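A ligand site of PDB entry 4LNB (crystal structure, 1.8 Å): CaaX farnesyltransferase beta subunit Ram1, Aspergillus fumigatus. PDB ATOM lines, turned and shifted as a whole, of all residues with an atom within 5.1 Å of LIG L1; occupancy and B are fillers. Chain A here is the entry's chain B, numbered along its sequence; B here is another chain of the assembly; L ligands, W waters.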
ATOM      1  N   TRP A 153      -0.751   7.706  -1.381  1.00  0.00           N
ATOM      2  CA  TRP A 153      -1.154   6.868  -2.509  1.00  0.00           C
ATOM      3  C   TRP A 153      -2.347   5.992  -2.136  1.00  0.00           C
ATOM      4  O   TRP A 153      -3.259   5.791  -2.934  1.00  0.00           O
ATOM      5  CB  TRP A 153      -0.014   5.967  -2.975  1.00  0.00           C
ATOM      6  CG  TRP A 153       0.953   6.598  -3.919  1.00  0.00           C
ATOM      7  CD1 TRP A 153       2.302   6.742  -3.747  1.00  0.00           C
ATOM      8  CD2 TRP A 153       0.658   7.137  -5.217  1.00  0.00           C
ATOM      9  NE1 TRP A 153       2.854   7.348  -4.846  1.00  0.00           N
ATOM     10  CE2 TRP A 153       1.877   7.603  -5.756  1.00  0.00           C
ATOM     11  CE3 TRP A 153      -0.510   7.283  -5.964  1.00  0.00           C
ATOM     12  CZ2 TRP A 153       1.956   8.199  -7.015  1.00  0.00           C
ATOM     13  CZ3 TRP A 153      -0.432   7.882  -7.214  1.00  0.00           C
ATOM     14  CH2 TRP A 153       0.794   8.324  -7.724  1.00  0.00           C
ATOM     15  N   TYR A 204       1.330  14.694  -5.595  1.00  0.00           N
ATOM     16  CA  TYR A 204       0.424  14.348  -6.694  1.00  0.00           C
ATOM     17  C   TYR A 204      -0.790  13.593  -6.139  1.00  0.00           C
ATOM     18  O   TYR A 204      -1.938  13.965  -6.411  1.00  0.00           O
ATOM     19  CB  TYR A 204       1.181  13.507  -7.716  1.00  0.00           C
ATOM     20  CG  TYR A 204       0.383  12.793  -8.782  1.00  0.00           C
ATOM     21  CD1 TYR A 204       0.119  13.403 -10.006  1.00  0.00           C
ATOM     22  CD2 TYR A 204      -0.061  11.491  -8.585  1.00  0.00           C
ATOM     23  CE1 TYR A 204      -0.589  12.730 -11.007  1.00  0.00           C
ATOM     24  CE2 TYR A 204      -0.759  10.820  -9.577  1.00  0.00           C
ATOM     25  CZ  TYR A 204      -1.013  11.448 -10.774  1.00  0.00           C
ATOM     26  OH  TYR A 204      -1.714  10.761 -11.750  1.00  0.00           O
ATOM     27  N   ARG A 252       8.640  10.159 -14.139  1.00  0.00           N
ATOM     28  CA  ARG A 252       7.571  10.141 -13.147  1.00  0.00           C
ATOM     29  C   ARG A 252       7.601  11.441 -12.353  1.00  0.00           C
ATOM     30  O   ARG A 252       6.569  12.043 -12.073  1.00  0.00           O
ATOM     31  CB  ARG A 252       7.753   8.936 -12.213  1.00  0.00           C
ATOM     32  CG  ARG A 252       7.089   9.103 -10.855  1.00  0.00           C
ATOM     33  CD  ARG A 252       7.551   8.042  -9.872  1.00  0.00           C
ATOM     34  NE  ARG A 252       8.999   8.084  -9.654  1.00  0.00           N
ATOM     35  CZ  ARG A 252       9.594   7.762  -8.507  1.00  0.00           C
ATOM     36  NH1 ARG A 252       8.863   7.376  -7.472  1.00  0.00           N
ATOM     37  NH2 ARG A 252      10.910   7.825  -8.405  1.00  0.00           N
ATOM     38  N   TYR A 255       6.206  14.325 -14.602  1.00  0.00           N
ATOM     39  CA  TYR A 255       4.750  14.231 -14.751  1.00  0.00           C
ATOM     40  C   TYR A 255       4.021  14.644 -13.471  1.00  0.00           C
ATOM     41  O   TYR A 255       3.086  15.452 -13.513  1.00  0.00           O
ATOM     42  CB  TYR A 255       4.344  12.812 -15.166  1.00  0.00           C
ATOM     43  CG  TYR A 255       2.870  12.529 -14.976  1.00  0.00           C
ATOM     44  CD1 TYR A 255       1.924  13.072 -15.827  1.00  0.00           C
ATOM     45  CD2 TYR A 255       2.424  11.703 -13.942  1.00  0.00           C
ATOM     46  CE1 TYR A 255       0.564  12.815 -15.651  1.00  0.00           C
ATOM     47  CE2 TYR A 255       1.083  11.435 -13.761  1.00  0.00           C
ATOM     48  CZ  TYR A 255       0.158  11.995 -14.617  1.00  0.00           C
ATOM     49  OH  TYR A 255      -1.182  11.739 -14.430  1.00  0.00           O
ATOM     50  N   CYS A 256       4.448  14.117 -12.329  1.00  0.00           N
ATOM     51  CA  CYS A 256       3.822  14.433 -11.057  1.00  0.00           C
ATOM     52  C   CYS A 256       3.948  15.925 -10.738  1.00  0.00           C
ATOM     53  O   CYS A 256       2.979  16.552 -10.317  1.00  0.00           O
ATOM     54  CB  CYS A 256       4.414  13.604  -9.921  1.00  0.00           C
ATOM     55  SG  CYS A 256       3.937  11.854  -9.965  1.00  0.00           S
ATOM     56  N   HIS A 311       9.413   1.622 -21.144  1.00  0.00           N
ATOM     57  CA  HIS A 311       8.432   1.047 -20.227  1.00  0.00           C
ATOM     58  C   HIS A 311       7.110   1.789 -20.274  1.00  0.00           C
ATOM     59  O   HIS A 311       7.074   3.018 -20.288  1.00  0.00           O
ATOM     60  CB  HIS A 311       8.965   1.040 -18.792  1.00  0.00           C
ATOM     61  CG  HIS A 311       8.245   0.085 -17.896  1.00  0.00           C
ATOM     62  ND1 HIS A 311       6.969   0.315 -17.437  1.00  0.00           N
ATOM     63  CD2 HIS A 311       8.626  -1.100 -17.380  1.00  0.00           C
ATOM     64  CE1 HIS A 311       6.585  -0.696 -16.679  1.00  0.00           C
ATOM     65  NE2 HIS A 311       7.573  -1.570 -16.625  1.00  0.00           N
ATOM     66  N   ALA A 313       4.769   2.461 -18.106  1.00  0.00           N
ATOM     67  CA  ALA A 313       4.464   3.432 -17.055  1.00  0.00           C
ATOM     68  C   ALA A 313       5.109   4.777 -17.352  1.00  0.00           C
ATOM     69  O   ALA A 313       4.502   5.838 -17.146  1.00  0.00           O
ATOM     70  CB  ALA A 313       4.908   2.905 -15.704  1.00  0.00           C
ATOM     71  N   TYR A 314       6.334   4.737 -17.861  1.00  0.00           N
ATOM     72  CA  TYR A 314       7.051   5.957 -18.200  1.00  0.00           C
ATOM     73  C   TYR A 314       6.551   6.567 -19.506  1.00  0.00           C
ATOM     74  O   TYR A 314       6.595   7.787 -19.692  1.00  0.00           O
ATOM     75  CB  TYR A 314       8.550   5.676 -18.268  1.00  0.00           C
ATOM     76  CG  TYR A 314       9.148   5.298 -16.925  1.00  0.00           C
ATOM     77  CD1 TYR A 314       8.902   6.078 -15.793  1.00  0.00           C
ATOM     78  CD2 TYR A 314       9.928   4.156 -16.786  1.00  0.00           C
ATOM     79  CE1 TYR A 314       9.459   5.732 -14.566  1.00  0.00           C
ATOM     80  CE2 TYR A 314      10.486   3.820 -15.562  1.00  0.00           C
ATOM     81  CZ  TYR A 314      10.242   4.601 -14.461  1.00  0.00           C
ATOM     82  OH  TYR A 314      10.781   4.263 -13.248  1.00  0.00           O
ATOM     83  N   CYS A 317       3.658   8.707 -18.428  1.00  0.00           N
ATOM     84  CA  CYS A 317       4.151   9.918 -17.768  1.00  0.00           C
ATOM     85  C   CYS A 317       4.643  10.949 -18.769  1.00  0.00           C
ATOM     86  O   CYS A 317       4.294  12.127 -18.674  1.00  0.00           O
ATOM     87  CB  CYS A 317       5.278   9.573 -16.793  1.00  0.00           C
ATOM     88  SG  CYS A 317       4.727   8.671 -15.321  1.00  0.00           S
ATOM     89  N   GLY A 358       4.313  -4.261 -19.569  1.00  0.00           N
ATOM     90  CA  GLY A 358       4.965  -2.970 -19.419  1.00  0.00           C
ATOM     91  C   GLY A 358       6.182  -2.787 -20.300  1.00  0.00           C
ATOM     92  O   GLY A 358       6.532  -1.669 -20.685  1.00  0.00           O
ATOM     93  N   ARG A 359       6.844  -3.880 -20.630  1.00  0.00           N
ATOM     94  CA  ARG A 359       8.020  -3.811 -21.488  1.00  0.00           C
ATOM     95  C   ARG A 359       8.210  -5.105 -22.255  1.00  0.00           C
ATOM     96  O   ARG A 359       7.610  -6.127 -21.920  1.00  0.00           O
ATOM     97  CB  ARG A 359       9.277  -3.455 -20.683  1.00  0.00           C
ATOM     98  CG  ARG A 359       9.405  -4.165 -19.349  1.00  0.00           C
ATOM     99  CD  ARG A 359      10.736  -3.852 -18.664  1.00  0.00           C
ATOM    100  NE  ARG A 359      10.706  -4.231 -17.261  1.00  0.00           N
ATOM    101  CZ  ARG A 359      11.780  -4.565 -16.543  1.00  0.00           C
ATOM    102  NH1 ARG A 359      12.981  -4.566 -17.106  1.00  0.00           N
ATOM    103  NH2 ARG A 359      11.640  -4.905 -15.260  1.00  0.00           N
ATOM    104  N   LYS A 362       8.261  -9.170 -21.168  1.00  0.00           N
ATOM    105  CA  LYS A 362       7.785  -9.386 -19.799  1.00  0.00           C
ATOM    106  C   LYS A 362       6.291  -9.697 -19.810  1.00  0.00           C
ATOM    107  O   LYS A 362       5.708  -9.887 -20.872  1.00  0.00           O
ATOM    108  CB  LYS A 362       8.158  -8.223 -18.887  1.00  0.00           C
ATOM    109  CG  LYS A 362       9.674  -8.035 -18.754  1.00  0.00           C
ATOM    110  CD  LYS A 362      10.093  -7.532 -17.375  1.00  0.00           C
ATOM    111  CE  LYS A 362       9.984  -8.628 -16.319  1.00  0.00           C
ATOM    112  NZ  LYS A 362      10.196  -8.083 -14.940  1.00  0.00           N
ATOM    113  N   LEU A 363       5.661  -9.747 -18.634  1.00  0.00           N
ATOM    114  CA  LEU A 363       4.309 -10.307 -18.521  1.00  0.00           C
ATOM    115  C   LEU A 363       3.188  -9.264 -18.476  1.00  0.00           C
ATOM    116  O   LEU A 363       3.411  -8.115 -18.078  1.00  0.00           O
ATOM    117  CB  LEU A 363       4.207 -11.205 -17.295  1.00  0.00           C
ATOM    118  CG  LEU A 363       5.239 -12.326 -17.142  1.00  0.00           C
ATOM    119  CD1 LEU A 363       5.150 -12.947 -15.761  1.00  0.00           C
ATOM    120  CD2 LEU A 363       5.046 -13.382 -18.227  1.00  0.00           C
ATOM    121  N   ASP A 365      -0.061  -7.355 -17.005  1.00  0.00           N
ATOM    122  CA  ASP A 365      -0.350  -6.911 -15.644  1.00  0.00           C
ATOM    123  C   ASP A 365      -1.509  -5.936 -15.736  1.00  0.00           C
ATOM    124  O   ASP A 365      -1.491  -5.005 -16.535  1.00  0.00           O
ATOM    125  CB  ASP A 365       0.907  -6.231 -15.054  1.00  0.00           C
ATOM    126  CG  ASP A 365       0.685  -5.673 -13.643  1.00  0.00           C
ATOM    127  OD1 ASP A 365      -0.469  -5.456 -13.218  1.00  0.00           O
ATOM    128  OD2 ASP A 365       1.698  -5.433 -12.957  1.00  0.00           O
ATOM    129  N   TYR A 368      -1.361  -2.009 -15.999  1.00  0.00           N
ATOM    130  CA  TYR A 368      -0.999  -1.392 -17.265  1.00  0.00           C
ATOM    131  C   TYR A 368      -2.229  -1.117 -18.127  1.00  0.00           C
ATOM    132  O   TYR A 368      -2.138  -0.452 -19.156  1.00  0.00           O
ATOM    133  CB  TYR A 368       0.044  -2.226 -18.027  1.00  0.00           C
ATOM    134  CG  TYR A 368       1.330  -2.385 -17.251  1.00  0.00           C
ATOM    135  CD1 TYR A 368       1.903  -1.301 -16.601  1.00  0.00           C
ATOM    136  CD2 TYR A 368       1.940  -3.626 -17.118  1.00  0.00           C
ATOM    137  CE1 TYR A 368       3.073  -1.430 -15.869  1.00  0.00           C
ATOM    138  CE2 TYR A 368       3.119  -3.766 -16.383  1.00  0.00           C
ATOM    139  CZ  TYR A 368       3.676  -2.667 -15.759  1.00  0.00           C
ATOM    140  OH  TYR A 368       4.835  -2.805 -15.025  1.00  0.00           O
ATOM    141  N   TRP A 371      -1.633   2.429 -17.388  1.00  0.00           N
ATOM    142  CA  TRP A 371      -0.378   3.020 -17.849  1.00  0.00           C
ATOM    143  C   TRP A 371      -0.210   2.942 -19.358  1.00  0.00           C
ATOM    144  O   TRP A 371       0.174   3.915 -20.000  1.00  0.00           O
ATOM    145  CB  TRP A 371       0.833   2.408 -17.134  1.00  0.00           C
ATOM    146  CG  TRP A 371       0.748   2.514 -15.641  1.00  0.00           C
ATOM    147  CD1 TRP A 371       0.636   1.484 -14.752  1.00  0.00           C
ATOM    148  CD2 TRP A 371       0.711   3.719 -14.872  1.00  0.00           C
ATOM    149  NE1 TRP A 371       0.567   1.975 -13.471  1.00  0.00           N
ATOM    150  CE2 TRP A 371       0.595   3.346 -13.516  1.00  0.00           C
ATOM    151  CE3 TRP A 371       0.776   5.074 -15.194  1.00  0.00           C
ATOM    152  CZ2 TRP A 371       0.549   4.283 -12.487  1.00  0.00           C
ATOM    153  CZ3 TRP A 371       0.720   6.013 -14.166  1.00  0.00           C
ATOM    154  CH2 TRP A 371       0.612   5.602 -12.828  1.00  0.00           C
ATOM    155  N   TYR A 432      -3.915  -0.692  -5.232  1.00  0.00           N
ATOM    156  CA  TYR A 432      -3.212  -0.129  -6.385  1.00  0.00           C
ATOM    157  C   TYR A 432      -3.710  -0.783  -7.667  1.00  0.00           C
ATOM    158  O   TYR A 432      -4.084  -0.103  -8.634  1.00  0.00           O
ATOM    159  CB  TYR A 432      -1.688  -0.316  -6.240  1.00  0.00           C
ATOM    160  CG  TYR A 432      -0.898  -0.128  -7.526  1.00  0.00           C
ATOM    161  CD1 TYR A 432      -0.446   1.122  -7.926  1.00  0.00           C
ATOM    162  CD2 TYR A 432      -0.597  -1.216  -8.341  1.00  0.00           C
ATOM    163  CE1 TYR A 432       0.276   1.288  -9.102  1.00  0.00           C
ATOM    164  CE2 TYR A 432       0.122  -1.069  -9.512  1.00  0.00           C
ATOM    165  CZ  TYR A 432       0.554   0.188  -9.894  1.00  0.00           C
ATOM    166  OH  TYR A 432       1.262   0.326 -11.063  1.00  0.00           O
ATOM    167  N   LYS B 159      16.182  -9.019 -14.977  1.00  0.00           N
ATOM    168  CA  LYS B 159      15.514  -7.886 -15.623  1.00  0.00           C
ATOM    169  C   LYS B 159      15.231  -6.717 -14.675  1.00  0.00           C
ATOM    170  O   LYS B 159      14.443  -5.821 -15.001  1.00  0.00           O
ATOM    171  CB  LYS B 159      14.221  -8.335 -16.296  1.00  0.00           C
ATOM    172  CG  LYS B 159      14.442  -9.443 -17.308  1.00  0.00           C
ATOM    173  CD  LYS B 159      13.165  -9.842 -18.017  1.00  0.00           C
ATOM    174  CE  LYS B 159      13.421 -10.983 -18.986  1.00  0.00           C
ATOM    175  NZ  LYS B 159      12.198 -11.289 -19.784  1.00  0.00           N
ATOM    176  N   TYR B 161      14.760  -3.524 -13.111  1.00  0.00           N
ATOM    177  CA  TYR B 161      14.812  -2.221 -13.783  1.00  0.00           C
ATOM    178  C   TYR B 161      15.753  -1.264 -13.080  1.00  0.00           C
ATOM    179  O   TYR B 161      16.509  -0.544 -13.735  1.00  0.00           O
ATOM    180  CB  TYR B 161      13.411  -1.610 -13.876  1.00  0.00           C
ATOM    181  CG  TYR B 161      13.297  -0.519 -14.918  1.00  0.00           C
ATOM    182  CD1 TYR B 161      12.851  -0.803 -16.208  1.00  0.00           C
ATOM    183  CD2 TYR B 161      13.662   0.802 -14.631  1.00  0.00           C
ATOM    184  CE1 TYR B 161      12.743   0.188 -17.166  1.00  0.00           C
ATOM    185  CE2 TYR B 161      13.574   1.790 -15.588  1.00  0.00           C
ATOM    186  CZ  TYR B 161      13.115   1.485 -16.851  1.00  0.00           C
ATOM    187  OH  TYR B 161      13.016   2.462 -17.816  1.00  0.00           O
HETATM  188  C1  LIG L   1       9.403  -2.104 -13.168  1.00  0.00           C
HETATM  189  O1  LIG L   1       8.907  -2.978 -12.205  1.00  0.00           O
HETATM  190  C2  LIG L   1       8.593  -1.039 -13.568  1.00  0.00           C
HETATM  191  C3  LIG L   1       9.052   0.400 -13.482  1.00  0.00           C
HETATM  192  C4  LIG L   1      10.499   0.475 -13.054  1.00  0.00           C
HETATM  193  C5  LIG L   1       8.147   1.221 -12.543  1.00  0.00           C
HETATM  194  C6  LIG L   1       7.094   2.112 -13.149  1.00  0.00           C
HETATM  195  C7  LIG L   1       6.474   3.100 -12.356  1.00  0.00           C
HETATM  196  C8  LIG L   1       5.061   2.928 -11.852  1.00  0.00           C
HETATM  197  C9  LIG L   1       4.447   1.632 -12.313  1.00  0.00           C
HETATM  198  C10 LIG L   1       4.180   4.088 -12.273  1.00  0.00           C
HETATM  199  C11 LIG L   1       4.716   5.491 -12.037  1.00  0.00           C
HETATM  200  C12 LIG L   1       3.970   6.583 -12.464  1.00  0.00           C
HETATM  201  C13 LIG L   1       3.730   7.762 -11.538  1.00  0.00           C
HETATM  202  C14 LIG L   1       3.933   7.439 -10.080  1.00  0.00           C
HETATM  203  C15 LIG L   1       2.487   8.533 -11.842  1.00  0.00           C
HETATM  204  P1  LIG L   1       8.655  -4.495 -12.479  1.00  0.00           P
HETATM  205  O2  LIG L   1       9.880  -5.184 -13.049  1.00  0.00           O
HETATM  206  O3  LIG L   1       8.297  -5.139 -11.163  1.00  0.00           O
HETATM  207  O4  LIG L   1       7.406  -4.636 -13.435  1.00  0.00           O
HETATM  208  P2  LIG L   1       7.415  -5.152 -14.919  1.00  0.00           P
HETATM  209  O5  LIG L   1       8.306  -4.282 -15.762  1.00  0.00           O
HETATM  210  O6  LIG L   1       5.996  -5.062 -15.417  1.00  0.00           O
HETATM  211  O7  LIG L   1       7.870  -6.588 -14.962  1.00  0.00           O
HETATM  212  O1  LG2 L   2       0.324  -5.658  -1.745  1.00  0.00           O
HETATM  213  C1  LG2 L   2       0.752  -4.555  -1.462  1.00  0.00           C
HETATM  214  O2  LG2 L   2       1.015  -4.242  -0.104  1.00  0.00           O
HETATM  215  C2  LG2 L   2       1.981  -4.950   0.694  1.00  0.00           C
HETATM  216  C3  LG2 L   2       2.531  -4.010   1.691  1.00  0.00           C
HETATM  217  C4  LG2 L   2       1.377  -6.100   1.404  1.00  0.00           C
HETATM  218  C5  LG2 L   2       3.130  -5.456  -0.197  1.00  0.00           C
HETATM  219  N1  LG2 L   2       1.351  -3.737  -2.540  1.00  0.00           N
HETATM  220  C6  LG2 L   2       1.457  -4.223  -3.926  1.00  0.00           C
HETATM  221  C7  LG2 L   2       0.928  -3.241  -4.918  1.00  0.00           C
HETATM  222  C8  LG2 L   2       1.873  -2.393  -2.328  1.00  0.00           C
HETATM  223  C9  LG2 L   2       1.378  -1.391  -3.346  1.00  0.00           C
HETATM  224  C10 LG2 L   2       1.485  -1.883  -4.751  1.00  0.00           C
HETATM  225  C11 LG2 L   2       2.964  -1.850  -5.210  1.00  0.00           C
HETATM  226  N2  LG2 L   2       3.692  -0.517  -5.071  1.00  0.00           N
HETATM  227  S1  LG2 L   2       5.321  -0.741  -4.733  1.00  0.00           S
HETATM  228  O3  LG2 L   2       6.109   0.357  -5.241  1.00  0.00           O
HETATM  229  O4  LG2 L   2       5.779  -1.962  -5.345  1.00  0.00           O
HETATM  230  C12 LG2 L   2       5.519  -0.897  -2.971  1.00  0.00           C
HETATM  231  C13 LG2 L   2       5.998  -2.103  -2.456  1.00  0.00           C
HETATM  232  C14 LG2 L   2       6.167  -2.282  -1.054  1.00  0.00           C
HETATM  233  C15 LG2 L   2       5.848  -1.247  -0.181  1.00  0.00           C
HETATM  234  C16 LG2 L   2       5.358  -0.038  -0.687  1.00  0.00           C
HETATM  235  C17 LG2 L   2       5.190   0.141  -2.088  1.00  0.00           C
HETATM  236  C18 LG2 L   2       4.667   1.455  -2.575  1.00  0.00           C
HETATM  237  C19 LG2 L   2       3.422   0.426  -6.240  1.00  0.00           C
HETATM  238  C20 LG2 L   2       3.518  -0.111  -7.694  1.00  0.00           C
HETATM  239  N3  LG2 L   2       4.832  -0.527  -8.199  1.00  0.00           N
HETATM  240  C21 LG2 L   2       5.906   0.498  -8.402  1.00  0.00           C
HETATM  241  C22 LG2 L   2       7.239   0.093  -8.553  1.00  0.00           C
HETATM  242  C23 LG2 L   2       8.247   1.056  -8.740  1.00  0.00           C
HETATM  243  C24 LG2 L   2       5.582   1.865  -8.437  1.00  0.00           C
HETATM  244  C25 LG2 L   2       6.580   2.831  -8.615  1.00  0.00           C
HETATM  245  C26 LG2 L   2       7.912   2.414  -8.773  1.00  0.00           C
HETATM  246  C27 LG2 L   2       8.966   3.446  -8.958  1.00  0.00           C
HETATM  247  N4  LG2 L   2       9.906   4.359  -9.090  1.00  0.00           N
HETATM  248  C28 LG2 L   2       5.094  -1.943  -8.517  1.00  0.00           C
HETATM  249  C29 LG2 L   2       4.305  -2.512  -9.689  1.00  0.00           C
HETATM  250  C30 LG2 L   2       3.097  -3.198  -9.627  1.00  0.00           C
HETATM  251  N5  LG2 L   2       2.746  -3.513 -10.883  1.00  0.00           N
HETATM  252  C31 LG2 L   2       3.673  -3.028 -11.700  1.00  0.00           C
HETATM  253  N6  LG2 L   2       4.625  -2.412 -10.976  1.00  0.00           N
HETATM  254  C32 LG2 L   2       5.819  -1.763 -11.509  1.00  0.00           C
HETATM  255  O   HOH W   1       4.232  -6.306 -13.653  1.00  0.00           O
HETATM  256  O   HOH W   2       5.419  -6.196 -17.853  1.00  0.00           O
HETATM  257  O   HOH W   3       8.410  -3.507  -8.835  1.00  0.00           O
HETATM  258  O   HOH W   4       6.445  -8.890 -15.865  1.00  0.00           O
HETATM  259  O   HOH W   5       6.978  -7.993 -12.740  1.00  0.00           O
HETATM  260  O   HOH W   6       5.626  -5.937 -10.690  1.00  0.00           O
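The side-chain hydroxyl (OH) of Tyr 368 lies within hydrogen-bond range of an oxygen (O6) of LIG L1 (2.6 Å).
The side-chain amino group of Lys 362 lies within salt-bridge range of an oxygen (O7) of LIG L1, 2.8 Å away.
NE of Arg 359 is in salt-bridge range of O5 of LIG L1 (2.8 Å).
An oxygen (O5) of LIG L1 sits at hydrogen-bond distance from a ring nitrogen (NE2) of His 311 (2.9 Å).
The side-chain hydroxyl (OH) of Tyr 368 lies close to a ring nitrogen (NE2) of His 311.
The guanidinium group (NH1) of Arg 359 is in hydrogen-bond range of the backbone carbonyl oxygen (O) of Lys 159 of chain B (2.9 Å).
ND1 of His 311 is in hydrogen-bond range of N of Ala 313 (3.1 Å).
The backbone carbonyl oxygen (O) of Ala 313 is in hydrogen-bond range of the side-chain sulfur (SG) of Cys 317 (3.4 Å).
The indole nitrogen of Trp 371 sits at hydrogen-bond distance from the side-chain hydroxyl of Tyr 432 (3.0 Å).
The side-chain sulfur of Cys 256 sits at hydrogen-bond distance from the backbone carbonyl oxygen of Arg 252 (3.4 Å).
OH of Tyr 255 is in hydrogen-bond range of OH of Tyr 204, at 2.9 Å.
Water W2 lies within hydrogen-bond range of an oxygen (O6) of LIG L1 (2.7 Å), the backbone carbonyl oxygen (O) of Leu 363 (2.8 Å) and the backbone NH (N) of Gly 358 (2.8 Å).
Water W4 bridges O7 of LIG L1 (2.9 Å) and N of Leu 363 (3.0 Å).
CZ2 of Trp 153 touches C14 of LIG L1, 3.7 Å away.
CG of Arg 252 touches C14 of LIG L1, 3.7 Å away.
Tyr 255 touches LIG L1 (CE2 to C15, 3.8 Å).
Ala 313 touches LIG L1.
Tyr 314 touches LIG L1 (OH to C4, 3.8 Å).
Cys 317 touches LIG L1 (SG to C12, 3.6 Å).
CH2 of Trp 371 touches C12 of LIG L1, 3.5 Å away.
Tyr 432 touches LIG L1.
Tyr 161 of chain B touches LIG L1 (CG to C4, 3.5 Å).
Hydrophobic or aromatic side chains that line LIG L1: Trp 153, Tyr 255, His 311, Ala 313, Tyr 368, Trp 371 and Tyr 161 of chain B.
13 residues have an atom within 4 Å of LIG L1: Trp 153, Arg 252, Tyr 255, His 311, Ala 313, Tyr 314, Cys 317, Arg 359, Lys 362, Tyr 368, Trp 371, Tyr 432 and Tyr 161 of chain B.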
